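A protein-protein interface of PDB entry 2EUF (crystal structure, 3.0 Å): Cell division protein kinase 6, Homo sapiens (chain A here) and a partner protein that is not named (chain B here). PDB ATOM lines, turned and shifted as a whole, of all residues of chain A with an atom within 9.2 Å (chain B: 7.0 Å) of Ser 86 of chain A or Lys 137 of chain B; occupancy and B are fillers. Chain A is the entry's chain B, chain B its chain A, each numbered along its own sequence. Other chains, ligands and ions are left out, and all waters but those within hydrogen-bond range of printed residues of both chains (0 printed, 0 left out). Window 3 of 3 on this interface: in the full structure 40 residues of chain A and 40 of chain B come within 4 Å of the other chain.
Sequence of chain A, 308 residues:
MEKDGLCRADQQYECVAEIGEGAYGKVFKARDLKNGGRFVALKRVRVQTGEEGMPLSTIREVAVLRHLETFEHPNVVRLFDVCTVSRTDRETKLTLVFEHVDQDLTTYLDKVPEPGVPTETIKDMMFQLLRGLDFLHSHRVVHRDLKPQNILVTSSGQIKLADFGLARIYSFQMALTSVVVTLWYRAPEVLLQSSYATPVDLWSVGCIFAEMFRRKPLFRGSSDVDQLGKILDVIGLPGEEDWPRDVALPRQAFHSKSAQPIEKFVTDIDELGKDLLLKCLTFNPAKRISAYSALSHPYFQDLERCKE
Of the 16 printed residues of chain B, 6 touch a printed residue of chain A.
Printed residues of chain B that touch a printed residue of chain A: Ile 133, Glu 136, Lys 137, Leu 140, Glu 141 and Trp 145.
Hydrophobic or aromatic side chains of chain B that line the printed part of chain A: Ile 133, Leu 140 and Trp 145.
Of the 20 printed residues of chain A, 6 touch a printed residue of chain B.
Among the printed residues, no Asp or Glu carboxylate lies within 4 Å of a Lys or Arg side-chain nitrogen of the other chain.
No residue of chain A comes within 4 Å of Asp 138 of chain B.
Of the printed residues of chain B, Ile 59 of chain A touches Leu 140 and Trp 145.
Of the printed residues of chain A, Ile 133 of chain B touches Gly 53 (3.98 Å).
Asn 134 of chain B touches none of the printed residues of chain A.
Leu 132 of chain B touches none of the printed residues of chain A.
The nearest residue of chain B that does not touch Ser 86 of chain A is Glu 141 of chain B (5.9 Å).
The nearest printed residue of chain A that does not touch Ile 133 of chain B is Glu 52 of chain A (4.5 Å).
The side-chain carboxylate (OE1) of Glu 136 of chain B is in hydrogen-bond range of the backbone NH (N) of Met 54 of chain A (2.7 Å).
The side-chain amino group (NZ) of Lys 137 of chain B is in hydrogen-bond range of the side-chain hydroxyl (OG) of Ser 86 of chain A (3.3 Å).
Ile 133 of chain B touches Gly 53 of chain A.
CA of Gly 53 of chain A touches OE1 of Glu 136 of chain B (3.5 Å).
Leu 140 of chain B touches Met 54 of chain A.
Met 54 of chain A touches Trp 145 of chain B (CE to CH2, 3.6 Å).
Ile 59 of chain A touches Leu 140 of chain B (CD1 to CD1, 3.8 Å).
CZ3 of Trp 145 of chain B touches CG1 of Ile 59 of chain A, 3.8 Å away.
Trp 145 of chain B touches Val 82 of chain A (NE1 to CG1, 3.6 Å).
Thr 84 of chain A touches Glu 141 of chain B.
The backbone carbonyl oxygen (O) of Leu 140 of chain B is in hydrogen-bond range of the backbone NH (N) of Trp 145 of chain B, 2.6 Å away.
OD1 of Asn 134 of chain B lies within hydrogen-bond range of NZ of Lys 137 of chain B (3.4 Å).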
ATOM      1  N   ASP A  10       3.267 -25.137 -24.841  1.00  0.00           N
ATOM      2  CA  ASP A  10       3.295 -26.628 -24.897  1.00  0.00           C
ATOM      3  C   ASP A  10       4.204 -27.191 -26.012  1.00  0.00           C
ATOM      4  O   ASP A  10       4.928 -28.169 -25.790  1.00  0.00           O
ATOM      5  CB  ASP A  10       1.870 -27.188 -25.012  1.00  0.00           C
ATOM      6  N   VAL A  47       4.815 -33.997 -11.319  1.00  0.00           N
ATOM      7  CA  VAL A  47       3.971 -33.982 -10.126  1.00  0.00           C
ATOM      8  C   VAL A  47       3.350 -35.349  -9.920  1.00  0.00           C
ATOM      9  O   VAL A  47       2.563 -35.818 -10.748  1.00  0.00           O
ATOM     10  CB  VAL A  47       2.837 -32.938 -10.227  1.00  0.00           C
ATOM     11  CG1 VAL A  47       1.956 -32.961  -8.970  1.00  0.00           C
ATOM     12  CG2 VAL A  47       3.401 -31.547 -10.464  1.00  0.00           C
ATOM     13  N   THR A  49       0.897 -37.938  -9.011  1.00  0.00           N
ATOM     14  CA  THR A  49      -0.548 -38.055  -8.779  1.00  0.00           C
ATOM     15  C   THR A  49      -0.851 -38.804  -7.477  1.00  0.00           C
ATOM     16  O   THR A  49      -1.735 -39.670  -7.431  1.00  0.00           O
ATOM     17  CB  THR A  49      -1.304 -38.703  -9.982  1.00  0.00           C
ATOM     18  OG1 THR A  49      -0.379 -39.344 -10.871  1.00  0.00           O
ATOM     19  CG2 THR A  49      -1.959 -37.634 -10.843  1.00  0.00           C
ATOM     20  N   GLU A  52      -0.840 -34.179  -2.979  1.00  0.00           N
ATOM     21  CA  GLU A  52      -0.315 -33.032  -2.236  1.00  0.00           C
ATOM     22  C   GLU A  52      -0.405 -31.716  -3.012  1.00  0.00           C
ATOM     23  O   GLU A  52      -0.119 -30.658  -2.462  1.00  0.00           O
ATOM     24  CB  GLU A  52       1.129 -33.272  -1.753  1.00  0.00           C
ATOM     25  CG  GLU A  52       1.314 -34.338  -0.663  1.00  0.00           C
ATOM     26  CD  GLU A  52       0.358 -34.217   0.534  1.00  0.00           C
ATOM     27  OE1 GLU A  52      -0.071 -33.087   0.872  1.00  0.00           O
ATOM     28  OE2 GLU A  52       0.030 -35.265   1.151  1.00  0.00           O
ATOM     29  N   GLY A  53      -0.813 -31.788  -4.279  1.00  0.00           N
ATOM     30  CA  GLY A  53      -0.847 -30.617  -5.153  1.00  0.00           C
ATOM     31  C   GLY A  53       0.553 -30.325  -5.637  1.00  0.00           C
ATOM     32  O   GLY A  53       1.429 -31.179  -5.519  1.00  0.00           O
ATOM     33  N   MET A  54       0.776 -29.126  -6.171  1.00  0.00           N
ATOM     34  CA  MET A  54       2.097 -28.762  -6.709  1.00  0.00           C
ATOM     35  C   MET A  54       3.165 -28.914  -5.643  1.00  0.00           C
ATOM     36  O   MET A  54       2.930 -28.578  -4.487  1.00  0.00           O
ATOM     37  CB  MET A  54       2.127 -27.330  -7.251  1.00  0.00           C
ATOM     38  CG  MET A  54       1.008 -26.979  -8.231  1.00  0.00           C
ATOM     39  SD  MET A  54       0.935 -28.010  -9.705  1.00  0.00           S
ATOM     40  CE  MET A  54       2.589 -27.767 -10.317  1.00  0.00           C
ATOM     41  N   ILE A  59       6.716 -24.453  -5.955  1.00  0.00           N
ATOM     42  CA  ILE A  59       5.871 -23.272  -5.750  1.00  0.00           C
ATOM     43  C   ILE A  59       6.684 -22.142  -5.139  1.00  0.00           C
ATOM     44  O   ILE A  59       6.685 -21.016  -5.647  1.00  0.00           O
ATOM     45  CB  ILE A  59       4.645 -23.606  -4.863  1.00  0.00           C
ATOM     46  CG1 ILE A  59       3.609 -24.370  -5.678  1.00  0.00           C
ATOM     47  CG2 ILE A  59       4.019 -22.338  -4.301  1.00  0.00           C
ATOM     48  CD1 ILE A  59       2.372 -24.706  -4.940  1.00  0.00           C
ATOM     49  N   VAL A  82       5.984 -20.529 -16.805  1.00  0.00           N
ATOM     50  CA  VAL A  82       5.541 -21.811 -16.260  1.00  0.00           C
ATOM     51  C   VAL A  82       4.430 -22.376 -17.140  1.00  0.00           C
ATOM     52  O   VAL A  82       3.336 -21.819 -17.211  1.00  0.00           O
ATOM     53  CB  VAL A  82       5.073 -21.707 -14.799  1.00  0.00           C
ATOM     54  CG1 VAL A  82       4.860 -23.095 -14.215  1.00  0.00           C
ATOM     55  CG2 VAL A  82       6.085 -20.954 -13.975  1.00  0.00           C
ATOM     56  N   CYS A  83       4.725 -23.484 -17.811  1.00  0.00           N
ATOM     57  CA  CYS A  83       3.816 -24.034 -18.802  1.00  0.00           C
ATOM     58  C   CYS A  83       2.532 -24.562 -18.168  1.00  0.00           C
ATOM     59  O   CYS A  83       1.457 -24.009 -18.413  1.00  0.00           O
ATOM     60  CB  CYS A  83       4.507 -25.108 -19.648  1.00  0.00           C
ATOM     61  N   THR A  84       2.655 -25.588 -17.322  1.00  0.00           N
ATOM     62  CA  THR A  84       1.505 -26.380 -16.821  1.00  0.00           C
ATOM     63  C   THR A  84       0.505 -26.831 -17.903  1.00  0.00           C
ATOM     64  O   THR A  84      -0.175 -26.010 -18.527  1.00  0.00           O
ATOM     65  CB  THR A  84       0.774 -25.741 -15.553  1.00  0.00           C
ATOM     66  OG1 THR A  84      -0.417 -26.485 -15.235  1.00  0.00           O
ATOM     67  CG2 THR A  84       0.258 -24.308 -15.805  1.00  0.00           C
ATOM     68  N   VAL A  85       0.441 -28.144 -18.116  1.00  0.00           N
ATOM     69  CA  VAL A  85      -0.610 -28.762 -18.936  1.00  0.00           C
ATOM     70  C   VAL A  85      -1.257 -29.925 -18.150  1.00  0.00           C
ATOM     71  O   VAL A  85      -0.668 -31.008 -18.018  1.00  0.00           O
ATOM     72  CB  VAL A  85      -0.089 -29.236 -20.346  1.00  0.00           C
ATOM     73  CG1 VAL A  85      -1.261 -29.556 -21.286  1.00  0.00           C
ATOM     74  CG2 VAL A  85       0.837 -28.196 -20.985  1.00  0.00           C
ATOM     75  N   SER A  86      -2.456 -29.688 -17.613  1.00  0.00           N
ATOM     76  CA  SER A  86      -3.175 -30.707 -16.842  1.00  0.00           C
ATOM     77  C   SER A  86      -3.596 -31.862 -17.743  1.00  0.00           C
ATOM     78  O   SER A  86      -4.080 -31.635 -18.852  1.00  0.00           O
ATOM     79  CB  SER A  86      -4.400 -30.098 -16.166  1.00  0.00           C
ATOM     80  OG  SER A  86      -4.047 -28.914 -15.479  1.00  0.00           O
ATOM     81  N   ARG A  87      -3.395 -33.094 -17.276  1.00  0.00           N
ATOM     82  CA  ARG A  87      -3.813 -34.274 -18.037  1.00  0.00           C
ATOM     83  C   ARG A  87      -4.911 -35.058 -17.315  1.00  0.00           C
ATOM     84  O   ARG A  87      -4.764 -35.419 -16.149  1.00  0.00           O
ATOM     85  CB  ARG A  87      -2.613 -35.175 -18.353  1.00  0.00           C
ATOM     86  N   THR A  88      -6.018 -35.299 -18.012  1.00  0.00           N
ATOM     87  CA  THR A  88      -7.076 -36.178 -17.507  1.00  0.00           C
ATOM     88  C   THR A  88      -6.803 -37.642 -17.891  1.00  0.00           C
ATOM     89  O   THR A  88      -7.445 -38.557 -17.363  1.00  0.00           O
ATOM     90  CB  THR A  88      -8.445 -35.721 -18.013  1.00  0.00           C
ATOM     91  N   ASP A  89      -5.850 -37.845 -18.809  1.00  0.00           N
ATOM     92  CA  ASP A  89      -5.380 -39.183 -19.214  1.00  0.00           C
ATOM     93  C   ASP A  89      -4.189 -39.653 -18.375  1.00  0.00           C
ATOM     94  O   ASP A  89      -3.881 -40.852 -18.339  1.00  0.00           O
ATOM     95  CB  ASP A  89      -4.966 -39.210 -20.694  1.00  0.00           C
ATOM     96  CG  ASP A  89      -6.009 -38.609 -21.616  1.00  0.00           C
ATOM     97  OD1 ASP A  89      -7.172 -38.434 -21.192  1.00  0.00           O
ATOM     98  OD2 ASP A  89      -5.749 -38.284 -22.796  1.00  0.00           O
ATOM     99  N   ARG A  90      -3.514 -38.705 -17.726  1.00  0.00           N
ATOM    100  CA  ARG A  90      -2.338 -38.987 -16.904  1.00  0.00           C
ATOM    101  C   ARG A  90      -2.181 -37.953 -15.785  1.00  0.00           C
ATOM    102  O   ARG A  90      -3.061 -37.125 -15.563  1.00  0.00           O
ATOM    103  CB  ARG A  90      -1.076 -39.036 -17.781  1.00  0.00           C
ATOM    104  N   GLU A  91      -1.062 -38.023 -15.072  1.00  0.00           N
ATOM    105  CA  GLU A  91      -0.680 -36.983 -14.127  1.00  0.00           C
ATOM    106  C   GLU A  91      -0.285 -35.715 -14.879  1.00  0.00           C
ATOM    107  O   GLU A  91      -0.065 -35.742 -16.092  1.00  0.00           O
ATOM    108  CB  GLU A  91       0.490 -37.460 -13.259  1.00  0.00           C
ATOM    109  CG  GLU A  91       1.787 -37.728 -14.018  1.00  0.00           C
ATOM    110  CD  GLU A  91       2.780 -38.586 -13.245  1.00  0.00           C
ATOM    111  OE1 GLU A  91       2.410 -39.160 -12.194  1.00  0.00           O
ATOM    112  OE2 GLU A  91       3.941 -38.695 -13.701  1.00  0.00           O
ATOM    113  N   THR A  92      -0.196 -34.605 -14.159  1.00  0.00           N
ATOM    114  CA  THR A  92       0.342 -33.384 -14.732  1.00  0.00           C
ATOM    115  C   THR A  92       1.854 -33.525 -14.924  1.00  0.00           C
ATOM    116  O   THR A  92       2.484 -34.417 -14.353  1.00  0.00           O
ATOM    117  CB  THR A  92       0.024 -32.190 -13.836  1.00  0.00           C
ATOM    118  N   LYS A  93       2.417 -32.657 -15.757  1.00  0.00           N
ATOM    119  CA  LYS A  93       3.860 -32.483 -15.867  1.00  0.00           C
ATOM    120  C   LYS A  93       4.102 -30.987 -16.045  1.00  0.00           C
ATOM    121  O   LYS A  93       3.238 -30.272 -16.560  1.00  0.00           O
ATOM    122  CB  LYS A  93       4.422 -33.281 -17.046  1.00  0.00           C
ATOM    123  N   LEU A  94       5.260 -30.505 -15.606  1.00  0.00           N
ATOM    124  CA  LEU A  94       5.557 -29.078 -15.693  1.00  0.00           C
ATOM    125  C   LEU A  94       6.756 -28.766 -16.562  1.00  0.00           C
ATOM    126  O   LEU A  94       7.776 -29.454 -16.496  1.00  0.00           O
ATOM    127  CB  LEU A  94       5.811 -28.488 -14.307  1.00  0.00           C
ATOM    128  CG  LEU A  94       4.662 -28.181 -13.343  1.00  0.00           C
ATOM    129  CD1 LEU A  94       5.263 -27.671 -12.043  1.00  0.00           C
ATOM    130  CD2 LEU A  94       3.684 -27.164 -13.920  1.00  0.00           C
ATOM    131  N   ALA B 100      -7.585 -23.367  -0.548  1.00  0.00           N
ATOM    132  CA  ALA B 100      -6.439 -23.481  -1.430  1.00  0.00           C
ATOM    133  C   ALA B 100      -5.413 -22.362  -1.165  1.00  0.00           C
ATOM    134  O   ALA B 100      -4.202 -22.528  -1.415  1.00  0.00           O
ATOM    135  CB  ALA B 100      -6.873 -23.519  -2.890  1.00  0.00           C
ATOM    136  N   ILE B 104      -1.644 -23.041  -0.303  1.00  0.00           N
ATOM    137  CA  ILE B 104      -0.528 -22.428  -1.023  1.00  0.00           C
ATOM    138  C   ILE B 104       0.370 -21.671  -0.034  1.00  0.00           C
ATOM    139  O   ILE B 104       1.593 -21.861  -0.023  1.00  0.00           O
ATOM    140  CB  ILE B 104      -0.988 -21.533  -2.227  1.00  0.00           C
ATOM    141  CG1 ILE B 104      -1.653 -22.382  -3.311  1.00  0.00           C
ATOM    142  CG2 ILE B 104       0.200 -20.870  -2.878  1.00  0.00           C
ATOM    143  CD1 ILE B 104      -2.305 -21.594  -4.434  1.00  0.00           C
ATOM    144  N   LEU B 130      -9.177 -33.973  -5.021  1.00  0.00           N
ATOM    145  CA  LEU B 130      -8.863 -33.744  -6.427  1.00  0.00           C
ATOM    146  C   LEU B 130      -9.287 -32.303  -6.738  1.00  0.00           C
ATOM    147  O   LEU B 130      -8.463 -31.473  -7.137  1.00  0.00           O
ATOM    148  CB  LEU B 130      -9.645 -34.735  -7.298  1.00  0.00           C
ATOM    149  CG  LEU B 130      -9.158 -35.143  -8.695  1.00  0.00           C
ATOM    150  CD1 LEU B 130     -10.248 -35.941  -9.428  1.00  0.00           C
ATOM    151  CD2 LEU B 130      -8.721 -33.947  -9.535  1.00  0.00           C
ATOM    152  N   LEU B 132      -9.797 -29.836  -4.971  1.00  0.00           N
ATOM    153  CA  LEU B 132      -9.016 -28.815  -4.283  1.00  0.00           C
ATOM    154  C   LEU B 132      -7.679 -28.598  -4.994  1.00  0.00           C
ATOM    155  O   LEU B 132      -7.244 -27.465  -5.167  1.00  0.00           O
ATOM    156  CB  LEU B 132      -8.815 -29.201  -2.814  1.00  0.00           C
ATOM    157  CG  LEU B 132      -8.463 -28.191  -1.695  1.00  0.00           C
ATOM    158  CD1 LEU B 132      -7.062 -28.418  -1.121  1.00  0.00           C
ATOM    159  CD2 LEU B 132      -8.699 -26.700  -2.041  1.00  0.00           C
ATOM    160  N   ILE B 133      -7.044 -29.684  -5.431  1.00  0.00           N
ATOM    161  CA  ILE B 133      -5.808 -29.592  -6.225  1.00  0.00           C
ATOM    162  C   ILE B 133      -5.930 -28.705  -7.486  1.00  0.00           C
ATOM    163  O   ILE B 133      -4.980 -27.995  -7.838  1.00  0.00           O
ATOM    164  CB  ILE B 133      -5.273 -31.013  -6.573  1.00  0.00           C
ATOM    165  CG1 ILE B 133      -4.685 -31.673  -5.318  1.00  0.00           C
ATOM    166  CG2 ILE B 133      -4.235 -30.957  -7.714  1.00  0.00           C
ATOM    167  CD1 ILE B 133      -4.549 -33.187  -5.404  1.00  0.00           C
ATOM    168  N   ASN B 134      -7.082 -28.745  -8.157  1.00  0.00           N
ATOM    169  CA  ASN B 134      -7.347 -27.834  -9.286  1.00  0.00           C
ATOM    170  C   ASN B 134      -7.434 -26.394  -8.817  1.00  0.00           C
ATOM    171  O   ASN B 134      -6.851 -25.487  -9.415  1.00  0.00           O
ATOM    172  CB  ASN B 134      -8.657 -28.179  -9.993  1.00  0.00           C
ATOM    173  CG  ASN B 134      -8.705 -29.598 -10.463  1.00  0.00           C
ATOM    174  OD1 ASN B 134      -7.709 -30.148 -10.938  1.00  0.00           O
ATOM    175  ND2 ASN B 134      -9.875 -30.213 -10.336  1.00  0.00           N
ATOM    176  N   GLN B 135      -8.172 -26.198  -7.735  1.00  0.00           N
ATOM    177  CA  GLN B 135      -8.386 -24.886  -7.196  1.00  0.00           C
ATOM    178  C   GLN B 135      -7.058 -24.287  -6.726  1.00  0.00           C
ATOM    179  O   GLN B 135      -6.997 -23.126  -6.306  1.00  0.00           O
ATOM    180  CB  GLN B 135      -9.397 -24.965  -6.059  1.00  0.00           C
ATOM    181  CG  GLN B 135      -9.722 -23.629  -5.439  1.00  0.00           C
ATOM    182  CD  GLN B 135     -10.286 -22.664  -6.451  1.00  0.00           C
ATOM    183  OE1 GLN B 135     -11.497 -22.633  -6.669  1.00  0.00           O
ATOM    184  NE2 GLN B 135      -9.415 -21.867  -7.069  1.00  0.00           N
ATOM    185  N   GLU B 136      -5.997 -25.092  -6.791  1.00  0.00           N
ATOM    186  CA  GLU B 136      -4.660 -24.624  -6.477  1.00  0.00           C
ATOM    187  C   GLU B 136      -4.038 -24.216  -7.784  1.00  0.00           C
ATOM    188  O   GLU B 136      -3.759 -23.039  -8.004  1.00  0.00           O
ATOM    189  CB  GLU B 136      -3.841 -25.727  -5.823  1.00  0.00           C
ATOM    190  CG  GLU B 136      -2.455 -25.291  -5.391  1.00  0.00           C
ATOM    191  CD  GLU B 136      -1.591 -26.452  -4.951  1.00  0.00           C
ATOM    192  OE1 GLU B 136      -1.115 -27.205  -5.831  1.00  0.00           O
ATOM    193  OE2 GLU B 136      -1.386 -26.605  -3.728  1.00  0.00           O
ATOM    194  N   LYS B 137      -3.834 -25.206  -8.648  1.00  0.00           N
ATOM    195  CA  LYS B 137      -3.452 -24.999 -10.034  1.00  0.00           C
ATOM    196  C   LYS B 137      -4.041 -23.698 -10.580  1.00  0.00           C
ATOM    197  O   LYS B 137      -3.300 -22.824 -11.011  1.00  0.00           O
ATOM    198  CB  LYS B 137      -3.958 -26.179 -10.845  1.00  0.00           C
ATOM    199  CG  LYS B 137      -3.095 -26.572 -12.012  1.00  0.00           C
ATOM    200  CD  LYS B 137      -3.120 -28.092 -12.237  1.00  0.00           C
ATOM    201  CE  LYS B 137      -4.464 -28.715 -11.828  1.00  0.00           C
ATOM    202  NZ  LYS B 137      -4.699 -30.064 -12.419  1.00  0.00           N
ATOM    203  N   ASP B 138      -5.371 -23.562 -10.508  1.00  0.00           N
ATOM    204  CA  ASP B 138      -6.103 -22.388 -11.021  1.00  0.00           C
ATOM    205  C   ASP B 138      -5.756 -21.056 -10.359  1.00  0.00           C
ATOM    206  O   ASP B 138      -5.771 -20.021 -11.022  1.00  0.00           O
ATOM    207  CB  ASP B 138      -7.605 -22.623 -10.952  1.00  0.00           C
ATOM    208  CG  ASP B 138      -8.057 -23.731 -11.876  1.00  0.00           C
ATOM    209  OD1 ASP B 138      -8.940 -24.517 -11.462  1.00  0.00           O
ATOM    210  OD2 ASP B 138      -7.585 -23.905 -13.029  1.00  0.00           O
ATOM    211  N   ILE B 139      -5.463 -21.067  -9.060  1.00  0.00           N
ATOM    212  CA  ILE B 139      -4.933 -19.867  -8.416  1.00  0.00           C
ATOM    213  C   ILE B 139      -3.512 -19.593  -8.931  1.00  0.00           C
ATOM    214  O   ILE B 139      -3.166 -18.451  -9.266  1.00  0.00           O
ATOM    215  CB  ILE B 139      -4.963 -19.965  -6.858  1.00  0.00           C
ATOM    216  CG1 ILE B 139      -6.403 -20.018  -6.341  1.00  0.00           C
ATOM    217  CG2 ILE B 139      -4.261 -18.769  -6.235  1.00  0.00           C
ATOM    218  CD1 ILE B 139      -6.533 -20.402  -4.873  1.00  0.00           C
ATOM    219  N   LEU B 140      -2.694 -20.639  -9.004  1.00  0.00           N
ATOM    220  CA  LEU B 140      -1.305 -20.466  -9.380  1.00  0.00           C
ATOM    221  C   LEU B 140      -1.177 -19.814 -10.748  1.00  0.00           C
ATOM    222  O   LEU B 140      -0.498 -18.807 -10.904  1.00  0.00           O
ATOM    223  CB  LEU B 140      -0.567 -21.798  -9.343  1.00  0.00           C
ATOM    224  CG  LEU B 140      -0.231 -22.267  -7.935  1.00  0.00           C
ATOM    225  CD1 LEU B 140       0.385 -23.648  -7.975  1.00  0.00           C
ATOM    226  CD2 LEU B 140       0.671 -21.255  -7.196  1.00  0.00           C
ATOM    227  N   GLU B 141      -1.860 -20.374 -11.734  1.00  0.00           N
ATOM    228  CA  GLU B 141      -1.751 -19.858 -13.083  1.00  0.00           C
ATOM    229  C   GLU B 141      -2.498 -18.543 -13.273  1.00  0.00           C
ATOM    230  O   GLU B 141      -2.140 -17.739 -14.129  1.00  0.00           O
ATOM    231  CB  GLU B 141      -2.172 -20.910 -14.114  1.00  0.00           C
ATOM    232  CG  GLU B 141      -3.494 -21.603 -13.826  1.00  0.00           C
ATOM    233  CD  GLU B 141      -3.896 -22.592 -14.916  1.00  0.00           C
ATOM    234  OE1 GLU B 141      -5.121 -22.819 -15.099  1.00  0.00           O
ATOM    235  OE2 GLU B 141      -2.993 -23.149 -15.592  1.00  0.00           O
ATOM    236  N   ALA B 142      -3.524 -18.317 -12.465  1.00  0.00           N
ATOM    237  CA  ALA B 142      -4.256 -17.060 -12.508  1.00  0.00           C
ATOM    238  C   ALA B 142      -3.350 -15.921 -12.081  1.00  0.00           C
ATOM    239  O   ALA B 142      -3.303 -14.886 -12.734  1.00  0.00           O
ATOM    240  CB  ALA B 142      -5.477 -17.126 -11.615  1.00  0.00           C
ATOM    241  N   LEU B 143      -2.628 -16.133 -10.984  1.00  0.00           N
ATOM    242  CA  LEU B 143      -1.691 -15.147 -10.443  1.00  0.00           C
ATOM    243  C   LEU B 143      -0.347 -15.227 -11.151  1.00  0.00           C
ATOM    244  O   LEU B 143       0.608 -14.530 -10.773  1.00  0.00           O
ATOM    245  CB  LEU B 143      -1.487 -15.379  -8.943  1.00  0.00           C
ATOM    246  CG  LEU B 143      -2.668 -15.108  -8.013  1.00  0.00           C
ATOM    247  CD1 LEU B 143      -2.325 -15.486  -6.598  1.00  0.00           C
ATOM    248  CD2 LEU B 143      -3.084 -13.642  -8.073  1.00  0.00           C
ATOM    249  N   TRP B 145       1.820 -17.611 -10.996  1.00  0.00           N
ATOM    250  CA  TRP B 145       2.805 -18.117 -10.040  1.00  0.00           C
ATOM    251  C   TRP B 145       3.505 -17.051  -9.195  1.00  0.00           C
ATOM    252  O   TRP B 145       4.364 -17.369  -8.367  1.00  0.00           O
ATOM    253  CB  TRP B 145       3.819 -19.001 -10.760  1.00  0.00           C
ATOM    254  CG  TRP B 145       3.227 -20.276 -11.216  1.00  0.00           C
ATOM    255  CD1 TRP B 145       2.369 -20.453 -12.266  1.00  0.00           C
ATOM    256  CD2 TRP B 145       3.431 -21.572 -10.645  1.00  0.00           C
ATOM    257  NE1 TRP B 145       2.031 -21.779 -12.384  1.00  0.00           N
ATOM    258  CE2 TRP B 145       2.667 -22.490 -11.398  1.00  0.00           C
ATOM    259  CE3 TRP B 145       4.196 -22.059  -9.578  1.00  0.00           C
ATOM    260  CZ2 TRP B 145       2.642 -23.861 -11.114  1.00  0.00           C
ATOM    261  CZ3 TRP B 145       4.168 -23.425  -9.298  1.00  0.00           C
ATOM    262  CH2 TRP B 145       3.392 -24.306 -10.061  1.00  0.00           C
